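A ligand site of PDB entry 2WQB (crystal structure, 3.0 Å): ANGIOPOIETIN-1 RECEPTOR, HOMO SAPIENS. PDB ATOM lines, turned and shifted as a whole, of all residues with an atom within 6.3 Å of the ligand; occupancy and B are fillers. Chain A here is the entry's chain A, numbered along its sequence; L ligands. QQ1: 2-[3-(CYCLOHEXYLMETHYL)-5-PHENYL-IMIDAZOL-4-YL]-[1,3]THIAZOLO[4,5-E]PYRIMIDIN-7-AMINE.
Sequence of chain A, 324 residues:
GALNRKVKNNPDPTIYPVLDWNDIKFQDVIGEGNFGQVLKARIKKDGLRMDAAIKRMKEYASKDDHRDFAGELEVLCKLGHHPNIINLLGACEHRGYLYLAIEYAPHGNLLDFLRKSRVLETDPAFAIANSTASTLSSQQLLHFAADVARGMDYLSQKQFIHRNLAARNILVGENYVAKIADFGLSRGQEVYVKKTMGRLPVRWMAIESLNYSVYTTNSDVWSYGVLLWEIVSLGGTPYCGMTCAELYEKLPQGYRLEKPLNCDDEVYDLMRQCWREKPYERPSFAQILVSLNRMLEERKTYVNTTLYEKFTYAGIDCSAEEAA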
ATOM      1  N   ILE A  30     -13.683   5.207  23.925  1.00  0.00           N
ATOM      2  CA  ILE A  30     -14.246   6.510  23.554  1.00  0.00           C
ATOM      3  C   ILE A  30     -14.709   6.531  22.089  1.00  0.00           C
ATOM      4  O   ILE A  30     -13.962   6.170  21.190  1.00  0.00           O
ATOM      5  CB  ILE A  30     -13.285   7.697  23.921  1.00  0.00           C
ATOM      6  CG1 ILE A  30     -11.894   7.562  23.267  1.00  0.00           C
ATOM      7  CG2 ILE A  30     -13.160   7.811  25.445  1.00  0.00           C
ATOM      8  CD1 ILE A  30     -10.761   8.214  24.075  1.00  0.00           C
ATOM      9  N   GLY A  36     -12.530   4.799  13.846  1.00  0.00           N
ATOM     10  CA  GLY A  36     -12.536   3.374  14.083  1.00  0.00           C
ATOM     11  C   GLY A  36     -12.611   3.028  15.570  1.00  0.00           C
ATOM     12  O   GLY A  36     -13.440   3.587  16.306  1.00  0.00           O
ATOM     13  N   VAL A  38     -11.265   3.162  19.234  1.00  0.00           N
ATOM     14  CA  VAL A  38     -10.350   3.925  20.140  1.00  0.00           C
ATOM     15  C   VAL A  38     -10.681   3.895  21.640  1.00  0.00           C
ATOM     16  O   VAL A  38     -11.823   3.739  22.025  1.00  0.00           O
ATOM     17  CB  VAL A  38     -10.096   5.424  19.684  1.00  0.00           C
ATOM     18  CG1 VAL A  38     -10.221   5.552  18.181  1.00  0.00           C
ATOM     19  CG2 VAL A  38     -10.987   6.383  20.390  1.00  0.00           C
ATOM     20  N   LEU A  39      -9.628   4.103  22.438  1.00  0.00           N
ATOM     21  CA  LEU A  39      -9.595   3.864  23.884  1.00  0.00           C
ATOM     22  C   LEU A  39      -8.796   4.911  24.648  1.00  0.00           C
ATOM     23  O   LEU A  39      -7.824   5.479  24.134  1.00  0.00           O
ATOM     24  CB  LEU A  39      -8.865   2.547  24.165  1.00  0.00           C
ATOM     25  CG  LEU A  39      -9.477   1.168  23.944  1.00  0.00           C
ATOM     26  CD1 LEU A  39      -8.979   0.556  22.646  1.00  0.00           C
ATOM     27  CD2 LEU A  39      -9.089   0.332  25.142  1.00  0.00           C
ATOM     28  N   ALA A  52      -3.262   9.087  27.201  1.00  0.00           N
ATOM     29  CA  ALA A  52      -3.148   8.995  25.777  1.00  0.00           C
ATOM     30  C   ALA A  52      -4.507   8.583  25.314  1.00  0.00           C
ATOM     31  O   ALA A  52      -5.333   8.175  26.120  1.00  0.00           O
ATOM     32  CB  ALA A  52      -2.130   7.968  25.408  1.00  0.00           C
ATOM     33  N   ALA A  53      -4.758   8.743  24.015  1.00  0.00           N
ATOM     34  CA  ALA A  53      -5.820   8.065  23.326  1.00  0.00           C
ATOM     35  C   ALA A  53      -5.107   7.092  22.397  1.00  0.00           C
ATOM     36  O   ALA A  53      -4.215   7.504  21.669  1.00  0.00           O
ATOM     37  CB  ALA A  53      -6.669   9.051  22.527  1.00  0.00           C
ATOM     38  N   ILE A  54      -5.477   5.820  22.449  1.00  0.00           N
ATOM     39  CA  ILE A  54      -4.814   4.787  21.679  1.00  0.00           C
ATOM     40  C   ILE A  54      -5.801   4.222  20.650  1.00  0.00           C
ATOM     41  O   ILE A  54      -6.913   3.819  21.008  1.00  0.00           O
ATOM     42  CB  ILE A  54      -4.335   3.639  22.577  1.00  0.00           C
ATOM     43  CG1 ILE A  54      -3.722   4.140  23.904  1.00  0.00           C
ATOM     44  CG2 ILE A  54      -3.363   2.749  21.831  1.00  0.00           C
ATOM     45  CD1 ILE A  54      -2.273   4.547  23.854  1.00  0.00           C
ATOM     46  N   LYS A  55      -5.406   4.209  19.386  1.00  0.00           N
ATOM     47  CA  LYS A  55      -6.167   3.523  18.322  1.00  0.00           C
ATOM     48  C   LYS A  55      -5.355   2.375  17.751  1.00  0.00           C
ATOM     49  O   LYS A  55      -4.163   2.508  17.486  1.00  0.00           O
ATOM     50  CB  LYS A  55      -6.558   4.492  17.188  1.00  0.00           C
ATOM     51  CG  LYS A  55      -7.655   3.942  16.206  1.00  0.00           C
ATOM     52  CD  LYS A  55      -7.727   4.703  14.849  1.00  0.00           C
ATOM     53  CE  LYS A  55      -8.977   4.297  14.034  1.00  0.00           C
ATOM     54  NZ  LYS A  55      -9.359   5.309  13.011  1.00  0.00           N
ATOM     55  N   MET A  57      -4.556  -0.061  14.856  1.00  0.00           N
ATOM     56  CA  MET A  57      -4.658  -0.287  13.405  1.00  0.00           C
ATOM     57  C   MET A  57      -4.230  -1.695  12.936  1.00  0.00           C
ATOM     58  O   MET A  57      -3.302  -2.305  13.483  1.00  0.00           O
ATOM     59  CB  MET A  57      -3.838   0.768  12.651  1.00  0.00           C
ATOM     60  CG  MET A  57      -4.518   2.115  12.605  1.00  0.00           C
ATOM     61  SD  MET A  57      -3.616   3.404  13.495  1.00  0.00           S
ATOM     62  CE  MET A  57      -2.434   3.875  12.208  1.00  0.00           C
ATOM     63  N   ILE A  86      -2.787  18.043  17.811  1.00  0.00           N
ATOM     64  CA  ILE A  86      -2.751  16.807  18.567  1.00  0.00           C
ATOM     65  C   ILE A  86      -1.420  16.077  18.384  1.00  0.00           C
ATOM     66  O   ILE A  86      -1.104  15.634  17.280  1.00  0.00           O
ATOM     67  CB  ILE A  86      -3.921  15.897  18.141  1.00  0.00           C
ATOM     68  CG1 ILE A  86      -4.652  15.408  19.381  1.00  0.00           C
ATOM     69  CG2 ILE A  86      -3.448  14.806  17.288  1.00  0.00           C
ATOM     70  CD1 ILE A  86      -5.188  16.578  20.247  1.00  0.00           C
ATOM     71  N   LEU A 100      -1.483   3.070  18.217  1.00  0.00           N
ATOM     72  CA  LEU A 100      -0.998   4.447  18.075  1.00  0.00           C
ATOM     73  C   LEU A 100      -1.479   5.385  19.209  1.00  0.00           C
ATOM     74  O   LEU A 100      -2.652   5.719  19.279  1.00  0.00           O
ATOM     75  CB  LEU A 100      -1.524   4.933  16.732  1.00  0.00           C
ATOM     76  CG  LEU A 100      -1.178   6.318  16.199  1.00  0.00           C
ATOM     77  CD1 LEU A 100       0.314   6.454  16.002  1.00  0.00           C
ATOM     78  CD2 LEU A 100      -1.944   6.553  14.882  1.00  0.00           C
ATOM     79  N   ALA A 101      -0.581   5.817  20.087  1.00  0.00           N
ATOM     80  CA  ALA A 101      -0.919   6.676  21.232  1.00  0.00           C
ATOM     81  C   ALA A 101      -0.741   8.126  20.859  1.00  0.00           C
ATOM     82  O   ALA A 101       0.347   8.521  20.480  1.00  0.00           O
ATOM     83  CB  ALA A 101      -0.031   6.331  22.423  1.00  0.00           C
ATOM     84  N   ILE A 102      -1.781   8.928  20.969  1.00  0.00           N
ATOM     85  CA  ILE A 102      -1.659  10.356  20.648  1.00  0.00           C
ATOM     86  C   ILE A 102      -2.210  11.213  21.781  1.00  0.00           C
ATOM     87  O   ILE A 102      -3.008  10.740  22.570  1.00  0.00           O
ATOM     88  CB  ILE A 102      -2.398  10.720  19.345  1.00  0.00           C
ATOM     89  CG1 ILE A 102      -3.906  10.830  19.618  1.00  0.00           C
ATOM     90  CG2 ILE A 102      -2.153   9.683  18.287  1.00  0.00           C
ATOM     91  CD1 ILE A 102      -4.752  10.947  18.395  1.00  0.00           C
ATOM     92  N   GLU A 103      -1.775  12.470  21.853  1.00  0.00           N
ATOM     93  CA  GLU A 103      -2.177  13.376  22.931  1.00  0.00           C
ATOM     94  C   GLU A 103      -3.666  13.291  23.163  1.00  0.00           C
ATOM     95  O   GLU A 103      -4.428  13.344  22.199  1.00  0.00           O
ATOM     96  CB  GLU A 103      -1.774  14.818  22.575  1.00  0.00           C
ATOM     97  CG  GLU A 103      -2.558  15.905  23.298  1.00  0.00           C
ATOM     98  CD  GLU A 103      -1.968  17.307  23.089  1.00  0.00           C
ATOM     99  OE1 GLU A 103      -1.209  17.547  22.096  1.00  0.00           O
ATOM    100  OE2 GLU A 103      -2.278  18.156  23.970  1.00  0.00           O
ATOM    101  N   TYR A 104      -4.065  13.163  24.435  1.00  0.00           N
ATOM    102  CA  TYR A 104      -5.487  13.003  24.854  1.00  0.00           C
ATOM    103  C   TYR A 104      -6.184  14.330  25.122  1.00  0.00           C
ATOM    104  O   TYR A 104      -5.666  15.160  25.845  1.00  0.00           O
ATOM    105  CB  TYR A 104      -5.584  12.172  26.151  1.00  0.00           C
ATOM    106  CG  TYR A 104      -6.982  12.063  26.707  1.00  0.00           C
ATOM    107  CD1 TYR A 104      -7.986  11.337  26.031  1.00  0.00           C
ATOM    108  CD2 TYR A 104      -7.324  12.632  27.922  1.00  0.00           C
ATOM    109  CE1 TYR A 104      -9.257  11.210  26.508  1.00  0.00           C
ATOM    110  CE2 TYR A 104      -8.623  12.499  28.435  1.00  0.00           C
ATOM    111  CZ  TYR A 104      -9.586  11.787  27.704  1.00  0.00           C
ATOM    112  OH  TYR A 104     -10.876  11.662  28.169  1.00  0.00           O
ATOM    113  N   ALA A 105      -7.367  14.498  24.557  1.00  0.00           N
ATOM    114  CA  ALA A 105      -8.175  15.725  24.709  1.00  0.00           C
ATOM    115  C   ALA A 105      -9.283  15.500  25.730  1.00  0.00           C
ATOM    116  O   ALA A 105     -10.289  14.864  25.410  1.00  0.00           O
ATOM    117  CB  ALA A 105      -8.778  16.141  23.370  1.00  0.00           C
ATOM    118  N   PRO A 106      -9.121  16.025  26.957  1.00  0.00           N
ATOM    119  CA  PRO A 106     -10.080  15.934  28.052  1.00  0.00           C
ATOM    120  C   PRO A 106     -11.547  16.327  27.771  1.00  0.00           C
ATOM    121  O   PRO A 106     -12.431  15.843  28.469  1.00  0.00           O
ATOM    122  CB  PRO A 106      -9.527  16.948  29.047  1.00  0.00           C
ATOM    123  CG  PRO A 106      -8.144  16.936  28.834  1.00  0.00           C
ATOM    124  CD  PRO A 106      -7.965  16.835  27.363  1.00  0.00           C
ATOM    125  N   GLY A 108     -13.619  16.662  24.569  1.00  0.00           N
ATOM    126  CA  GLY A 108     -14.432  16.362  23.390  1.00  0.00           C
ATOM    127  C   GLY A 108     -14.107  17.259  22.224  1.00  0.00           C
ATOM    128  O   GLY A 108     -13.146  18.055  22.291  1.00  0.00           O
ATOM    129  N   ASN A 109     -14.867  17.106  21.126  1.00  0.00           N
ATOM    130  CA  ASN A 109     -14.741  17.998  19.975  1.00  0.00           C
ATOM    131  C   ASN A 109     -15.245  19.413  20.302  1.00  0.00           C
ATOM    132  O   ASN A 109     -16.084  19.584  21.186  1.00  0.00           O
ATOM    133  CB  ASN A 109     -15.516  17.432  18.788  1.00  0.00           C
ATOM    134  CG  ASN A 109     -17.013  17.617  18.911  1.00  0.00           C
ATOM    135  OD1 ASN A 109     -17.534  18.719  18.758  1.00  0.00           O
ATOM    136  ND2 ASN A 109     -17.704  16.543  19.187  1.00  0.00           N
ATOM    137  N   ARG A 168     -16.757  20.374  14.824  1.00  0.00           N
ATOM    138  CA  ARG A 168     -16.770  19.017  15.329  1.00  0.00           C
ATOM    139  C   ARG A 168     -15.425  18.334  15.118  1.00  0.00           C
ATOM    140  O   ARG A 168     -15.217  17.253  15.664  1.00  0.00           O
ATOM    141  CB  ARG A 168     -17.820  18.194  14.593  1.00  0.00           C
ATOM    142  CG  ARG A 168     -17.309  17.701  13.247  1.00  0.00           C
ATOM    143  CD  ARG A 168     -18.374  17.147  12.283  1.00  0.00           C
ATOM    144  NE  ARG A 168     -17.823  17.314  10.921  1.00  0.00           N
ATOM    145  CZ  ARG A 168     -18.328  18.070   9.952  1.00  0.00           C
ATOM    146  NH1 ARG A 168     -19.488  18.706  10.074  1.00  0.00           N
ATOM    147  NH2 ARG A 168     -17.656  18.155   8.795  1.00  0.00           N
ATOM    148  N   ASN A 169     -14.538  18.905  14.297  1.00  0.00           N
ATOM    149  CA  ASN A 169     -13.283  18.220  13.897  1.00  0.00           C
ATOM    150  C   ASN A 169     -12.038  18.783  14.574  1.00  0.00           C
ATOM    151  O   ASN A 169     -10.924  18.400  14.238  1.00  0.00           O
ATOM    152  CB  ASN A 169     -13.134  18.242  12.379  1.00  0.00           C
ATOM    153  CG  ASN A 169     -13.937  17.148  11.706  1.00  0.00           C
ATOM    154  OD1 ASN A 169     -14.279  16.159  12.332  1.00  0.00           O
ATOM    155  ND2 ASN A 169     -14.243  17.326  10.448  1.00  0.00           N
ATOM    156  N   ILE A 170     -12.291  19.638  15.560  1.00  0.00           N
ATOM    157  CA  ILE A 170     -11.296  20.268  16.395  1.00  0.00           C
ATOM    158  C   ILE A 170     -11.548  19.751  17.788  1.00  0.00           C
ATOM    159  O   ILE A 170     -12.705  19.710  18.242  1.00  0.00           O
ATOM    160  CB  ILE A 170     -11.510  21.788  16.381  1.00  0.00           C
ATOM    161  CG1 ILE A 170     -11.294  22.309  14.985  1.00  0.00           C
ATOM    162  CG2 ILE A 170     -10.587  22.479  17.279  1.00  0.00           C
ATOM    163  CD1 ILE A 170     -10.047  21.758  14.277  1.00  0.00           C
ATOM    164  N   LEU A 171     -10.475  19.369  18.482  1.00  0.00           N
ATOM    165  CA  LEU A 171     -10.572  18.872  19.838  1.00  0.00           C
ATOM    166  C   LEU A 171     -10.132  19.969  20.772  1.00  0.00           C
ATOM    167  O   LEU A 171      -9.228  20.743  20.461  1.00  0.00           O
ATOM    168  CB  LEU A 171      -9.650  17.690  20.035  1.00  0.00           C
ATOM    169  CG  LEU A 171      -9.960  16.370  19.339  1.00  0.00           C
ATOM    170  CD1 LEU A 171      -8.655  15.662  19.103  1.00  0.00           C
ATOM    171  CD2 LEU A 171     -10.881  15.470  20.141  1.00  0.00           C
ATOM    172  N   ALA A 181      -6.418  17.836  14.405  1.00  0.00           N
ATOM    173  CA  ALA A 181      -6.016  16.475  14.088  1.00  0.00           C
ATOM    174  C   ALA A 181      -5.183  16.436  12.795  1.00  0.00           C
ATOM    175  O   ALA A 181      -5.676  16.743  11.710  1.00  0.00           O
ATOM    176  CB  ALA A 181      -7.260  15.602  13.919  1.00  0.00           C
ATOM    177  N   PHE A 183      -4.213  13.744  11.010  1.00  0.00           N
ATOM    178  CA  PHE A 183      -4.218  12.454  10.256  1.00  0.00           C
ATOM    179  C   PHE A 183      -4.831  12.588   8.865  1.00  0.00           C
ATOM    180  O   PHE A 183      -5.780  13.350   8.664  1.00  0.00           O
ATOM    181  CB  PHE A 183      -4.931  11.294  10.982  1.00  0.00           C
ATOM    182  CG  PHE A 183      -5.070  11.470  12.445  1.00  0.00           C
ATOM    183  CD1 PHE A 183      -6.327  11.687  13.008  1.00  0.00           C
ATOM    184  CD2 PHE A 183      -3.956  11.450  13.269  1.00  0.00           C
ATOM    185  CE1 PHE A 183      -6.475  11.872  14.387  1.00  0.00           C
ATOM    186  CE2 PHE A 183      -4.089  11.643  14.651  1.00  0.00           C
ATOM    187  CZ  PHE A 183      -5.357  11.850  15.197  1.00  0.00           C
HETATM  188  C1  QQ1 L   1      -5.329   7.571  17.958  1.00  0.00           C
HETATM  189  C2  QQ1 L   1      -6.359   7.736  18.851  1.00  0.00           C
HETATM  190  C6  QQ1 L   1      -5.498   7.922  16.635  1.00  0.00           C
HETATM  191  C3  QQ1 L   1      -7.575   8.255  18.431  1.00  0.00           C
HETATM  192  C5  QQ1 L   1      -6.704   8.449  16.209  1.00  0.00           C
HETATM  193  C24 QQ1 L   1      -9.726  12.307  22.917  1.00  0.00           C
HETATM  194  C10 QQ1 L   1     -10.662   9.549  15.321  1.00  0.00           C
HETATM  195  C4  QQ1 L   1      -7.759   8.627  17.094  1.00  0.00           C
HETATM  196  C21 QQ1 L   1      -8.881  11.651  20.447  1.00  0.00           C
HETATM  197  C7  QQ1 L   1      -9.049   9.205  16.648  1.00  0.00           C
HETATM  198  C8  QQ1 L   1      -9.882  10.065  17.297  1.00  0.00           C
HETATM  199  C22 QQ1 L   1      -7.979  12.266  21.388  1.00  0.00           C
HETATM  200  C26 QQ1 L   1     -10.156  11.433  20.899  1.00  0.00           C
HETATM  201  C19 QQ1 L   1      -9.778  10.681  18.628  1.00  0.00           C
HETATM  202  C16 QQ1 L   1     -11.483  15.251  15.670  1.00  0.00           C
HETATM  203  C15 QQ1 L   1     -12.850  14.781  16.082  1.00  0.00           C
HETATM  204  C17 QQ1 L   1     -10.745  14.198  14.894  1.00  0.00           C
HETATM  205  C14 QQ1 L   1     -12.757  13.467  16.815  1.00  0.00           C
HETATM  206  C18 QQ1 L   1     -10.697  12.911  15.686  1.00  0.00           C
HETATM  207  C13 QQ1 L   1     -12.088  12.431  15.951  1.00  0.00           C
HETATM  208  C12 QQ1 L   1     -12.125  11.101  16.595  1.00  0.00           C
HETATM  209  N23 QQ1 L   1      -8.444  12.579  22.634  1.00  0.00           N
HETATM  210  N25 QQ1 L   1     -10.622  11.746  22.100  1.00  0.00           N
HETATM  211  N11 QQ1 L   1      -9.549   8.894  15.394  1.00  0.00           N
HETATM  212  N20 QQ1 L   1      -8.687  11.209  19.135  1.00  0.00           N
HETATM  213  N9  QQ1 L   1     -10.933  10.278  16.414  1.00  0.00           N
HETATM  214  N28 QQ1 L   1      -6.701  12.539  21.140  1.00  0.00           N
HETATM  215  S27 QQ1 L   1     -11.149  10.682  19.695  1.00  0.00           S
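O of Glu 103 is in hydrogen-bond range of N28 of the ligand, at 2.6 Å.
N of Ala 105 sits at hydrogen-bond distance from N23 of the ligand (2.9 Å).
The backbone carbonyl oxygen (O) of Lys 55 lies within hydrogen-bond range of the backbone NH (N) of Leu 100 (2.8 Å).
The backbone NH of Ile 102 sits at hydrogen-bond distance from the backbone carbonyl oxygen of Ala 53.
The backbone NH of Ile 30 sits at hydrogen-bond distance from the backbone carbonyl oxygen of Val 38 (3.0 Å).
The backbone NH (N) of Ile 54 is in hydrogen-bond range of the backbone carbonyl oxygen (O) of Leu 39.
Merely in contact with the ligand: Lys 55 (3.4 Å), Arg 168 (3.4 Å), Ile 102 (3.5 Å), Asn 169 (3.5 Å), Leu 100 (3.5 Å), Ala 53 (3.5 Å), Tyr 104 (3.6 Å), Val 38 (3.8 Å), Phe 183 (3.8 Å), Ala 181 (3.9 Å), Ile 86 (3.9 Å) and Ile 54 (3.99 Å).
Hydrophobic or aromatic side chains that line the ligand: Val 38, Ala 53, Ile 86, Ile 102, Tyr 104, Ala 105, Ala 181 and Phe 183.
Of the 25 residues printed, 14 come within 4 Å of the ligand.
The nearest printed residue that does not touch the ligand is Ile 30 (4.05 Å).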
